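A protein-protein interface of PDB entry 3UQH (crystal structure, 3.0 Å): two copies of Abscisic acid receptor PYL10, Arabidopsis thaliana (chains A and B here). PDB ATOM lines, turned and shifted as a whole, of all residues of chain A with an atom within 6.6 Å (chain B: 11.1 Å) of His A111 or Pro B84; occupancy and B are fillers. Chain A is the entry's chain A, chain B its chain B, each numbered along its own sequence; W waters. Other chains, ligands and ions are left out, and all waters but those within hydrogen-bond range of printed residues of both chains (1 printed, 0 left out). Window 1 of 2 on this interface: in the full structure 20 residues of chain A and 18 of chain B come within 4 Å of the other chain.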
ATOM      1  N   LEU A  79     -24.022   0.980  27.499  1.00  0.00           N
ATOM      2  CA  LEU A  79     -24.710  -0.266  27.209  1.00  0.00           C
ATOM      3  C   LEU A  79     -25.229  -0.885  28.498  1.00  0.00           C
ATOM      4  O   LEU A  79     -24.812  -0.505  29.591  1.00  0.00           O
ATOM      5  CB  LEU A  79     -23.777  -1.220  26.467  1.00  0.00           C
ATOM      6  CG  LEU A  79     -23.308  -0.662  25.118  1.00  0.00           C
ATOM      7  CD1 LEU A  79     -22.159  -1.447  24.543  1.00  0.00           C
ATOM      8  CD2 LEU A  79     -24.441  -0.614  24.131  1.00  0.00           C
ATOM      9  N   PRO A  84     -20.666  -7.729  25.631  1.00  0.00           N
ATOM     10  CA  PRO A  84     -19.224  -7.689  25.334  1.00  0.00           C
ATOM     11  C   PRO A  84     -18.602  -6.277  25.253  1.00  0.00           C
ATOM     12  O   PRO A  84     -17.378  -6.154  25.241  1.00  0.00           O
ATOM     13  CB  PRO A  84     -19.117  -8.407  23.973  1.00  0.00           C
ATOM     14  CG  PRO A  84     -20.417  -9.148  23.807  1.00  0.00           C
ATOM     15  CD  PRO A  84     -21.434  -8.307  24.509  1.00  0.00           C
ATOM     16  N   ALA A  85     -19.423  -5.232  25.188  1.00  0.00           N
ATOM     17  CA  ALA A  85     -18.919  -3.869  25.324  1.00  0.00           C
ATOM     18  C   ALA A  85     -19.799  -3.035  26.240  1.00  0.00           C
ATOM     19  O   ALA A  85     -20.995  -3.288  26.319  1.00  0.00           O
ATOM     20  CB  ALA A  85     -19.024  -3.133  24.019  1.00  0.00           C
ATOM     21  N   THR A  86     -19.220  -2.054  26.932  1.00  0.00           N
ATOM     22  CA  THR A  86     -19.996  -1.209  27.845  1.00  0.00           C
ATOM     23  C   THR A  86     -20.260   0.273  27.545  1.00  0.00           C
ATOM     24  O   THR A  86     -21.028   0.915  28.265  1.00  0.00           O
ATOM     25  CB  THR A  86     -19.292  -1.295  29.225  1.00  0.00           C
ATOM     26  OG1 THR A  86     -18.156  -0.433  29.244  1.00  0.00           O
ATOM     27  CG2 THR A  86     -18.855  -2.691  29.530  1.00  0.00           C
ATOM     28  N   LYS A  87     -19.628   0.829  26.517  1.00  0.00           N
ATOM     29  CA  LYS A  87     -19.776   2.264  26.254  1.00  0.00           C
ATOM     30  C   LYS A  87     -19.492   2.634  24.799  1.00  0.00           C
ATOM     31  O   LYS A  87     -18.668   2.003  24.140  1.00  0.00           O
ATOM     32  CB  LYS A  87     -18.902   3.086  27.222  1.00  0.00           C
ATOM     33  CG  LYS A  87     -17.398   2.853  27.069  1.00  0.00           C
ATOM     34  CD  LYS A  87     -16.582   3.387  28.243  1.00  0.00           C
ATOM     35  CE  LYS A  87     -15.096   3.143  28.003  1.00  0.00           C
ATOM     36  NZ  LYS A  87     -14.267   3.380  29.215  1.00  0.00           N
ATOM     37  N   SER A  88     -20.169   3.657  24.295  1.00  0.00           N
ATOM     38  CA  SER A  88     -19.924   4.116  22.935  1.00  0.00           C
ATOM     39  C   SER A  88     -20.031   5.632  22.855  1.00  0.00           C
ATOM     40  O   SER A  88     -20.920   6.233  23.464  1.00  0.00           O
ATOM     41  CB  SER A  88     -20.907   3.449  21.973  1.00  0.00           C
ATOM     42  OG  SER A  88     -20.806   3.966  20.664  1.00  0.00           O
ATOM     43  N   THR A  89     -19.116   6.246  22.113  1.00  0.00           N
ATOM     44  CA  THR A  89     -19.131   7.696  21.916  1.00  0.00           C
ATOM     45  C   THR A  89     -19.457   8.025  20.462  1.00  0.00           C
ATOM     46  O   THR A  89     -18.675   7.735  19.553  1.00  0.00           O
ATOM     47  CB  THR A  89     -17.792   8.352  22.352  1.00  0.00           C
ATOM     48  OG1 THR A  89     -17.572   8.109  23.746  1.00  0.00           O
ATOM     49  CG2 THR A  89     -17.816   9.852  22.110  1.00  0.00           C
ATOM     50  N   GLU A  90     -20.621   8.631  20.256  1.00  0.00           N
ATOM     51  CA  GLU A  90     -21.151   8.854  18.913  1.00  0.00           C
ATOM     52  C   GLU A  90     -21.339  10.351  18.642  1.00  0.00           C
ATOM     53  O   GLU A  90     -21.427  11.138  19.573  1.00  0.00           O
ATOM     54  CB  GLU A  90     -22.444   8.048  18.731  1.00  0.00           C
ATOM     55  CG  GLU A  90     -22.285   6.567  19.156  1.00  0.00           C
ATOM     56  CD  GLU A  90     -23.596   5.773  19.261  1.00  0.00           C
ATOM     57  OE1 GLU A  90     -24.676   6.320  18.933  1.00  0.00           O
ATOM     58  OE2 GLU A  90     -23.540   4.583  19.672  1.00  0.00           O
ATOM     59  N   ILE A 106     -19.620   6.911  14.963  1.00  0.00           N
ATOM     60  CA  ILE A 106     -18.999   6.508  16.216  1.00  0.00           C
ATOM     61  C   ILE A 106     -17.519   6.913  16.208  1.00  0.00           C
ATOM     62  O   ILE A 106     -16.828   6.736  15.203  1.00  0.00           O
ATOM     63  CB  ILE A 106     -19.165   4.998  16.507  1.00  0.00           C
ATOM     64  CG1 ILE A 106     -20.639   4.610  16.517  1.00  0.00           C
ATOM     65  CG2 ILE A 106     -18.547   4.651  17.848  1.00  0.00           C
ATOM     66  CD1 ILE A 106     -20.901   3.241  17.071  1.00  0.00           C
ATOM     67  N   VAL A 107     -17.053   7.465  17.327  1.00  0.00           N
ATOM     68  CA  VAL A 107     -15.684   7.987  17.444  1.00  0.00           C
ATOM     69  C   VAL A 107     -14.934   7.463  18.672  1.00  0.00           C
ATOM     70  O   VAL A 107     -13.794   7.867  18.930  1.00  0.00           O
ATOM     71  CB  VAL A 107     -15.655   9.540  17.469  1.00  0.00           C
ATOM     72  CG1 VAL A 107     -15.921  10.118  16.078  1.00  0.00           C
ATOM     73  CG2 VAL A 107     -16.615  10.092  18.527  1.00  0.00           C
ATOM     74  N   GLY A 108     -15.576   6.570  19.421  1.00  0.00           N
ATOM     75  CA  GLY A 108     -14.967   5.966  20.604  1.00  0.00           C
ATOM     76  C   GLY A 108     -15.900   5.011  21.330  1.00  0.00           C
ATOM     77  O   GLY A 108     -17.020   4.744  20.866  1.00  0.00           O
ATOM     78  N   GLY A 109     -15.443   4.516  22.485  1.00  0.00           N
ATOM     79  CA  GLY A 109     -16.150   3.469  23.225  1.00  0.00           C
ATOM     80  C   GLY A 109     -15.353   2.176  23.202  1.00  0.00           C
ATOM     81  O   GLY A 109     -14.315   2.093  22.542  1.00  0.00           O
ATOM     82  N   ASP A 110     -15.830   1.159  23.907  1.00  0.00           N
ATOM     83  CA  ASP A 110     -15.015  -0.035  24.104  1.00  0.00           C
ATOM     84  C   ASP A 110     -15.458  -1.182  23.195  1.00  0.00           C
ATOM     85  O   ASP A 110     -15.048  -2.332  23.383  1.00  0.00           O
ATOM     86  CB  ASP A 110     -14.897  -0.397  25.602  1.00  0.00           C
ATOM     87  CG  ASP A 110     -16.241  -0.756  26.256  1.00  0.00           C
ATOM     88  OD1 ASP A 110     -17.320  -0.613  25.628  1.00  0.00           O
ATOM     89  OD2 ASP A 110     -16.203  -1.188  27.429  1.00  0.00           O
ATOM     90  N   HIS A 111     -16.275  -0.870  22.194  1.00  0.00           N
ATOM     91  CA  HIS A 111     -16.696  -1.870  21.215  1.00  0.00           C
ATOM     92  C   HIS A 111     -15.583  -2.106  20.198  1.00  0.00           C
ATOM     93  O   HIS A 111     -15.613  -3.065  19.427  1.00  0.00           O
ATOM     94  CB  HIS A 111     -17.975  -1.423  20.505  1.00  0.00           C
ATOM     95  CG  HIS A 111     -17.935  -0.005  20.025  1.00  0.00           C
ATOM     96  ND1 HIS A 111     -16.986   0.679  19.343  1.00  0.00           N
ATOM     97  CD2 HIS A 111     -18.968   0.882  20.237  1.00  0.00           C
ATOM     98  CE1 HIS A 111     -17.460   1.955  19.158  1.00  0.00           C
ATOM     99  NE2 HIS A 111     -18.657   2.052  19.706  1.00  0.00           N
ATOM    100  N   ARG A 112     -14.602  -1.211  20.214  1.00  0.00           N
ATOM    101  CA  ARG A 112     -13.431  -1.262  19.326  1.00  0.00           C
ATOM    102  C   ARG A 112     -13.810  -1.085  17.857  1.00  0.00           C
ATOM    103  O   ARG A 112     -13.000  -1.386  16.972  1.00  0.00           O
ATOM    104  CB  ARG A 112     -12.541  -2.508  19.474  1.00  0.00           C
ATOM    105  CG  ARG A 112     -11.515  -2.437  20.573  1.00  0.00           C
ATOM    106  CD  ARG A 112     -11.913  -3.342  21.675  1.00  0.00           C
ATOM    107  NE  ARG A 112     -10.933  -3.327  22.737  1.00  0.00           N
ATOM    108  CZ  ARG A 112     -11.086  -3.953  23.895  1.00  0.00           C
ATOM    109  NH1 ARG A 112     -12.187  -4.661  24.147  1.00  0.00           N
ATOM    110  NH2 ARG A 112     -10.130  -3.866  24.803  1.00  0.00           N
ATOM    111  N   LEU A 113     -15.023  -0.602  17.601  1.00  0.00           N
ATOM    112  CA  LEU A 113     -15.481  -0.345  16.232  1.00  0.00           C
ATOM    113  C   LEU A 113     -14.705   0.805  15.606  1.00  0.00           C
ATOM    114  O   LEU A 113     -14.642   1.889  16.171  1.00  0.00           O
ATOM    115  CB  LEU A 113     -16.977  -0.044  16.203  1.00  0.00           C
ATOM    116  CG  LEU A 113     -17.918  -1.239  16.295  1.00  0.00           C
ATOM    117  CD1 LEU A 113     -19.354  -0.733  16.277  1.00  0.00           C
ATOM    118  CD2 LEU A 113     -17.662  -2.256  15.162  1.00  0.00           C
ATOM    119  N   LYS A 114     -14.106   0.567  14.445  1.00  0.00           N
ATOM    120  CA  LYS A 114     -13.228   1.580  13.855  1.00  0.00           C
ATOM    121  C   LYS A 114     -13.790   2.209  12.573  1.00  0.00           C
ATOM    122  O   LYS A 114     -14.076   1.524  11.589  1.00  0.00           O
ATOM    123  CB  LYS A 114     -11.797   1.041  13.656  1.00  0.00           C
ATOM    124  CG  LYS A 114     -11.038   0.747  14.948  1.00  0.00           C
ATOM    125  CD  LYS A 114      -9.651   0.199  14.645  1.00  0.00           C
ATOM    126  CE  LYS A 114      -8.866  -0.078  15.920  1.00  0.00           C
ATOM    127  NZ  LYS A 114      -8.042  -1.318  15.795  1.00  0.00           N
ATOM    128  N   TYR A 116     -16.745   3.501  12.278  1.00  0.00           N
ATOM    129  CA  TYR A 116     -18.161   3.207  12.066  1.00  0.00           C
ATOM    130  C   TYR A 116     -18.906   4.477  11.687  1.00  0.00           C
ATOM    131  O   TYR A 116     -18.739   5.503  12.325  1.00  0.00           O
ATOM    132  CB  TYR A 116     -18.810   2.579  13.312  1.00  0.00           C
ATOM    133  CG  TYR A 116     -20.257   2.225  13.065  1.00  0.00           C
ATOM    134  CD1 TYR A 116     -20.616   0.958  12.597  1.00  0.00           C
ATOM    135  CD2 TYR A 116     -21.264   3.166  13.252  1.00  0.00           C
ATOM    136  CE1 TYR A 116     -21.943   0.637  12.339  1.00  0.00           C
ATOM    137  CE2 TYR A 116     -22.584   2.863  12.992  1.00  0.00           C
ATOM    138  CZ  TYR A 116     -22.921   1.600  12.531  1.00  0.00           C
ATOM    139  OH  TYR A 116     -24.242   1.299  12.273  1.00  0.00           O
ATOM    140  N   PRO A 144     -12.130  -5.496  11.378  1.00  0.00           N
ATOM    141  CA  PRO A 144     -11.068  -5.793  12.337  1.00  0.00           C
ATOM    142  C   PRO A 144      -9.938  -6.472  11.580  1.00  0.00           C
ATOM    143  O   PRO A 144     -10.202  -7.350  10.762  1.00  0.00           O
ATOM    144  CB  PRO A 144     -11.761  -6.808  13.240  1.00  0.00           C
ATOM    145  CG  PRO A 144     -13.190  -6.353  13.275  1.00  0.00           C
ATOM    146  CD  PRO A 144     -13.476  -5.687  11.965  1.00  0.00           C
ATOM    147  N   PHE B  58     -11.541 -15.931  15.684  1.00  0.00           N
ATOM    148  CA  PHE B  58     -11.399 -14.784  16.581  1.00  0.00           C
ATOM    149  C   PHE B  58     -10.347 -14.952  17.689  1.00  0.00           C
ATOM    150  O   PHE B  58     -10.069 -14.015  18.446  1.00  0.00           O
ATOM    151  CB  PHE B  58     -12.760 -14.383  17.151  1.00  0.00           C
ATOM    152  CG  PHE B  58     -13.800 -14.119  16.101  1.00  0.00           C
ATOM    153  CD1 PHE B  58     -13.611 -13.113  15.151  1.00  0.00           C
ATOM    154  CD2 PHE B  58     -14.976 -14.876  16.058  1.00  0.00           C
ATOM    155  CE1 PHE B  58     -14.566 -12.859  14.172  1.00  0.00           C
ATOM    156  CE2 PHE B  58     -15.944 -14.633  15.085  1.00  0.00           C
ATOM    157  CZ  PHE B  58     -15.736 -13.615  14.136  1.00  0.00           C
ATOM    158  N   ASP B  78      -6.610 -15.505  24.308  1.00  0.00           N
ATOM    159  CA  ASP B  78      -6.566 -14.111  23.897  1.00  0.00           C
ATOM    160  C   ASP B  78      -7.170 -13.960  22.517  1.00  0.00           C
ATOM    161  O   ASP B  78      -6.631 -14.494  21.557  1.00  0.00           O
ATOM    162  CB  ASP B  78      -5.143 -13.575  23.900  1.00  0.00           C
ATOM    163  CG  ASP B  78      -4.532 -13.548  25.293  1.00  0.00           C
ATOM    164  OD1 ASP B  78      -5.123 -12.911  26.207  1.00  0.00           O
ATOM    165  OD2 ASP B  78      -3.446 -14.157  25.468  1.00  0.00           O
ATOM    166  N   LEU B  79      -8.297 -13.250  22.436  1.00  0.00           N
ATOM    167  CA  LEU B  79      -8.906 -12.837  21.158  1.00  0.00           C
ATOM    168  C   LEU B  79      -8.021 -11.873  20.338  1.00  0.00           C
ATOM    169  O   LEU B  79      -6.959 -11.418  20.795  1.00  0.00           O
ATOM    170  CB  LEU B  79     -10.265 -12.164  21.387  1.00  0.00           C
ATOM    171  CG  LEU B  79     -11.413 -12.897  22.075  1.00  0.00           C
ATOM    172  CD1 LEU B  79     -12.680 -12.089  21.914  1.00  0.00           C
ATOM    173  CD2 LEU B  79     -11.600 -14.279  21.493  1.00  0.00           C
ATOM    174  N   LYS B  80      -8.484 -11.556  19.129  1.00  0.00           N
ATOM    175  CA  LYS B  80      -7.772 -10.654  18.226  1.00  0.00           C
ATOM    176  C   LYS B  80      -8.118  -9.187  18.471  1.00  0.00           C
ATOM    177  O   LYS B  80      -9.112  -8.855  19.124  1.00  0.00           O
ATOM    178  CB  LYS B  80      -8.050 -11.030  16.767  1.00  0.00           C
ATOM    179  CG  LYS B  80      -7.654 -12.457  16.418  1.00  0.00           C
ATOM    180  CD  LYS B  80      -7.953 -12.790  14.975  1.00  0.00           C
ATOM    181  CE  LYS B  80      -6.907 -13.732  14.406  1.00  0.00           C
ATOM    182  NZ  LYS B  80      -7.345 -14.271  13.095  1.00  0.00           N
ATOM    183  N   SER B  81      -7.282  -8.311  17.932  1.00  0.00           N
ATOM    184  CA  SER B  81      -7.456  -6.879  18.093  1.00  0.00           C
ATOM    185  C   SER B  81      -8.658  -6.366  17.327  1.00  0.00           C
ATOM    186  O   SER B  81      -8.940  -6.837  16.228  1.00  0.00           O
ATOM    187  CB  SER B  81      -6.207  -6.160  17.618  1.00  0.00           C
ATOM    188  OG  SER B  81      -5.123  -6.504  18.460  1.00  0.00           O
ATOM    189  N   GLY B  82      -9.363  -5.412  17.928  1.00  0.00           N
ATOM    190  CA  GLY B  82     -10.469  -4.738  17.275  1.00  0.00           C
ATOM    191  C   GLY B  82     -11.804  -5.436  17.379  1.00  0.00           C
ATOM    192  O   GLY B  82     -12.718  -5.125  16.618  1.00  0.00           O
ATOM    193  N   LEU B  83     -11.923  -6.378  18.310  1.00  0.00           N
ATOM    194  CA  LEU B  83     -13.193  -7.035  18.587  1.00  0.00           C
ATOM    195  C   LEU B  83     -13.783  -6.501  19.888  1.00  0.00           C
ATOM    196  O   LEU B  83     -13.050  -5.934  20.700  1.00  0.00           O
ATOM    197  CB  LEU B  83     -12.998  -8.543  18.666  1.00  0.00           C
ATOM    198  CG  LEU B  83     -12.433  -9.154  17.384  1.00  0.00           C
ATOM    199  CD1 LEU B  83     -12.154 -10.640  17.532  1.00  0.00           C
ATOM    200  CD2 LEU B  83     -13.389  -8.897  16.238  1.00  0.00           C
ATOM    201  N   PRO B  84     -15.110  -6.659  20.087  1.00  0.00           N
ATOM    202  CA  PRO B  84     -15.755  -6.256  21.348  1.00  0.00           C
ATOM    203  C   PRO B  84     -15.129  -6.834  22.626  1.00  0.00           C
ATOM    204  O   PRO B  84     -15.094  -6.156  23.649  1.00  0.00           O
ATOM    205  CB  PRO B  84     -17.183  -6.745  21.168  1.00  0.00           C
ATOM    206  CG  PRO B  84     -17.404  -6.597  19.687  1.00  0.00           C
ATOM    207  CD  PRO B  84     -16.111  -6.994  19.053  1.00  0.00           C
ATOM    208  N   ALA B  85     -14.616  -8.055  22.567  1.00  0.00           N
ATOM    209  CA  ALA B  85     -13.927  -8.629  23.721  1.00  0.00           C
ATOM    210  C   ALA B  85     -12.441  -8.938  23.453  1.00  0.00           C
ATOM    211  O   ALA B  85     -12.003  -8.943  22.297  1.00  0.00           O
ATOM    212  CB  ALA B  85     -14.662  -9.860  24.190  1.00  0.00           C
ATOM    213  N   THR B  86     -11.669  -9.183  24.516  1.00  0.00           N
ATOM    214  CA  THR B  86     -10.227  -9.455  24.388  1.00  0.00           C
ATOM    215  C   THR B  86      -9.742 -10.755  25.021  1.00  0.00           C
ATOM    216  O   THR B  86      -8.694 -11.269  24.631  1.00  0.00           O
ATOM    217  CB  THR B  86      -9.347  -8.340  24.979  1.00  0.00           C
ATOM    218  OG1 THR B  86      -9.612  -8.201  26.381  1.00  0.00           O
ATOM    219  CG2 THR B  86      -9.567  -7.033  24.258  1.00  0.00           C
ATOM    220  N   LYS B  87     -10.464 -11.268  26.010  1.00  0.00           N
ATOM    221  CA  LYS B  87     -10.020 -12.487  26.684  1.00  0.00           C
ATOM    222  C   LYS B  87     -11.163 -13.396  27.123  1.00  0.00           C
ATOM    223  O   LYS B  87     -12.281 -12.938  27.346  1.00  0.00           O
ATOM    224  CB  LYS B  87      -9.072 -12.164  27.855  1.00  0.00           C
ATOM    225  CG  LYS B  87      -9.617 -11.188  28.875  1.00  0.00           C
ATOM    226  CD  LYS B  87      -8.530 -10.667  29.794  1.00  0.00           C
ATOM    227  CE  LYS B  87      -9.073  -9.560  30.679  1.00  0.00           C
ATOM    228  NZ  LYS B  87      -7.993  -8.663  31.159  1.00  0.00           N
ATOM    229  N   SER B  88     -10.870 -14.687  27.222  1.00  0.00           N
ATOM    230  CA  SER B  88     -11.821 -15.666  27.728  1.00  0.00           C
ATOM    231  C   SER B  88     -11.070 -16.769  28.461  1.00  0.00           C
ATOM    232  O   SER B  88     -10.037 -17.247  27.996  1.00  0.00           O
ATOM    233  CB  SER B  88     -12.652 -16.259  26.586  1.00  0.00           C
ATOM    234  OG  SER B  88     -13.638 -17.153  27.072  1.00  0.00           O
ATOM    235  N   GLY B 109     -13.450 -14.030  31.699  1.00  0.00           N
ATOM    236  CA  GLY B 109     -13.122 -13.263  30.484  1.00  0.00           C
ATOM    237  C   GLY B 109     -14.004 -12.040  30.240  1.00  0.00           C
ATOM    238  O   GLY B 109     -15.179 -12.020  30.621  1.00  0.00           O
ATOM    239  N   ASP B 110     -13.452 -11.030  29.570  1.00  0.00           N
ATOM    240  CA  ASP B 110     -14.111  -9.726  29.459  1.00  0.00           C
ATOM    241  C   ASP B 110     -15.350  -9.674  28.549  1.00  0.00           C
ATOM    242  O   ASP B 110     -15.919  -8.597  28.370  1.00  0.00           O
ATOM    243  CB  ASP B 110     -13.091  -8.627  29.080  1.00  0.00           C
ATOM    244  CG  ASP B 110     -12.625  -8.710  27.619  1.00  0.00           C
ATOM    245  OD1 ASP B 110     -12.696  -9.792  26.988  1.00  0.00           O
ATOM    246  OD2 ASP B 110     -12.173  -7.672  27.096  1.00  0.00           O
ATOM    247  N   HIS B 111     -15.761 -10.816  27.988  1.00  0.00           N
ATOM    248  CA  HIS B 111     -16.943 -10.885  27.102  1.00  0.00           C
ATOM    249  C   HIS B 111     -18.247 -10.796  27.888  1.00  0.00           C
ATOM    250  O   HIS B 111     -19.307 -10.505  27.317  1.00  0.00           O
ATOM    251  CB  HIS B 111     -16.956 -12.169  26.261  1.00  0.00           C
ATOM    252  CG  HIS B 111     -16.752 -13.415  27.067  1.00  0.00           C
ATOM    253  ND1 HIS B 111     -17.320 -13.834  28.225  1.00  0.00           N
ATOM    254  CD2 HIS B 111     -15.831 -14.378  26.724  1.00  0.00           C
ATOM    255  CE1 HIS B 111     -16.743 -15.033  28.550  1.00  0.00           C
ATOM    256  NE2 HIS B 111     -15.854 -15.343  27.627  1.00  0.00           N
ATOM    257  N   ARG B 112     -18.158 -11.077  29.189  1.00  0.00           N
ATOM    258  CA  ARG B 112     -19.272 -10.917  30.138  1.00  0.00           C
ATOM    259  C   ARG B 112     -20.402 -11.957  29.999  1.00  0.00           C
ATOM    260  O   ARG B 112     -21.416 -11.877  30.719  1.00  0.00           O
ATOM    261  CB  ARG B 112     -19.801  -9.467  30.140  1.00  0.00           C
ATOM    262  CG  ARG B 112     -18.724  -8.465  30.495  1.00  0.00           C
ATOM    263  CD  ARG B 112     -19.237  -7.062  30.690  1.00  0.00           C
ATOM    264  NE  ARG B 112     -18.122  -6.157  30.970  1.00  0.00           N
ATOM    265  CZ  ARG B 112     -17.371  -5.554  30.042  1.00  0.00           C
ATOM    266  NH1 ARG B 112     -17.604  -5.725  28.740  1.00  0.00           N
ATOM    267  NH2 ARG B 112     -16.378  -4.763  30.420  1.00  0.00           N
ATOM    268  N   LEU B 113     -20.220 -12.927  29.094  1.00  0.00           N
ATOM    269  CA  LEU B 113     -21.104 -14.092  29.016  1.00  0.00           C
ATOM    270  C   LEU B 113     -21.061 -14.868  30.323  1.00  0.00           C
ATOM    271  O   LEU B 113     -19.982 -15.146  30.854  1.00  0.00           O
ATOM    272  CB  LEU B 113     -20.694 -15.033  27.890  1.00  0.00           C
ATOM    273  CG  LEU B 113     -20.881 -14.671  26.423  1.00  0.00           C
ATOM    274  CD1 LEU B 113     -20.189 -15.747  25.569  1.00  0.00           C
ATOM    275  CD2 LEU B 113     -22.346 -14.531  26.050  1.00  0.00           C
ATOM    276  N   PHE B 155     -26.760 -13.852  18.179  1.00  0.00           N
ATOM    277  CA  PHE B 155     -25.338 -13.480  18.180  1.00  0.00           C
ATOM    278  C   PHE B 155     -24.484 -14.687  18.544  1.00  0.00           C
ATOM    279  O   PHE B 155     -23.469 -14.947  17.893  1.00  0.00           O
ATOM    280  CB  PHE B 155     -25.037 -12.321  19.144  1.00  0.00           C
ATOM    281  CG  PHE B 155     -25.513 -10.982  18.662  1.00  0.00           C
ATOM    282  CD1 PHE B 155     -26.506 -10.293  19.355  1.00  0.00           C
ATOM    283  CD2 PHE B 155     -24.975 -10.409  17.513  1.00  0.00           C
ATOM    284  CE1 PHE B 155     -26.956  -9.055  18.915  1.00  0.00           C
ATOM    285  CE2 PHE B 155     -25.425  -9.172  17.060  1.00  0.00           C
ATOM    286  CZ  PHE B 155     -26.418  -8.492  17.765  1.00  0.00           C
ATOM    287  N   LEU B 159     -21.765 -16.642  16.076  1.00  0.00           N
ATOM    288  CA  LEU B 159     -20.367 -16.897  16.400  1.00  0.00           C
ATOM    289  C   LEU B 159     -20.024 -18.361  16.165  1.00  0.00           C
ATOM    290  O   LEU B 159     -19.071 -18.679  15.454  1.00  0.00           O
ATOM    291  CB  LEU B 159     -20.073 -16.513  17.851  1.00  0.00           C
ATOM    292  CG  LEU B 159     -18.609 -16.235  18.196  1.00  0.00           C
ATOM    293  CD1 LEU B 159     -18.481 -15.715  19.621  1.00  0.00           C
ATOM    294  CD2 LEU B 159     -17.764 -17.484  18.000  1.00  0.00           C
HETATM  295  O   HOH W   1     -15.532  -3.773  27.418  1.00  0.00           O
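The guanidinium group of Arg A112 lies within hydrogen-bond range of the backbone carbonyl oxygen of Pro B84, at 3.3 Å. O of Pro A84 lies close to O of Pro B84.
ND1 of His A111 is in hydrogen-bond range of N of Leu A113 (2.9 Å). O of Thr B86 lies within hydrogen-bond range of N of Leu B79. ND1 of His B111 sits close to N of Leu B113 (3.2 Å). The side-chain carboxylate of Asp A110 lies within hydrogen-bond range of the backbone NH of Lys A87 (2.9 Å). NE2 of His A111 sits close to O of Gly A108 (3.4 Å). NH1 of Arg B112 is in hydrogen-bond range of O of Asp B110 (3.4 Å).
CA of Pro A84 touches O of His B111, 3.4 Å away. Thr A86 touches Arg B112 (CG2 to CZ, 3.3 Å). O of Asp A110 touches O of Pro B84, at 3.8 Å. Leu B83 touches His A111 (C to O, 3.9 Å). Pro B84 touches His A111 (N to O, 3.7 Å). Gly B82 touches Arg A112 (C to CB, 3.7 Å). Leu B83 touches Arg A112 (O to CD, 3.0 Å). Arg A112 touches Thr B86. Gly B82 touches Pro A144. Pro A144 touches Leu B83 (CG to CD2, 3.9 Å).
Printed residues of chain B within 4 Å of Thr A86: Arg B112 (3.3 Å). No residue of chain B comes within 4 Å of Ser A88. Glu A90 touches none of the printed residues of chain B. No residue of chain B comes within 4 Å of Ile A106. No residue of chain B comes within 4 Å of Gly A108. No residue of chain B comes within 4 Å of Gly A109. Of chain B, only Leu B83 (3.9 Å) and Pro B84 (3.7 Å) come within 4 Å of His A111. Of chain B, only Gly B82, Leu B83, Pro B84 and Thr B86 come within 4 Å of Arg A112. No residue of chain B comes within 4 Å of Leu A113. Of the printed residues of chain A, Leu B83 touches His A111, Arg A112 and Pro A144. Lys B87 touches none of the printed residues of chain A. Of the printed residues of chain A, His B111 touches Pro A84. The nearest residue of chain B that does not touch His A111 is Gly B82 (4.5 Å). The nearest printed residue of chain B that does not touch Thr A86 is Pro B84 (6.7 Å).
Of the 19 printed residues of chain A, 6 touch a printed residue of chain B. Hydrophobic or aromatic side chains of chain A that line the printed part of chain B: Pro A84 and Pro A144. Hydrophobic or aromatic side chains of chain B within 4 Å of the printed part of chain A: Leu B83 and Pro B84. Among the printed residues, 13 pairs touch across the chains.
Pro A84 touches His B111, and with the chains exchanged His A111 touches Pro B84. Pro A84 touches Arg B112, and with the chains exchanged Arg A112 touches Pro B84. Thr A86 touches Arg B112, and with the chains exchanged Arg A112 touches Thr B86. Asp A110 touches Pro B84, but with the chains exchanged Pro A84 does not touch Asp B110 (4.2 Å).
Water W1 lies within hydrogen-bond range of OD2 of Asp A110 (2.7 Å) and NH1 of Arg B112 (3.1 Å).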
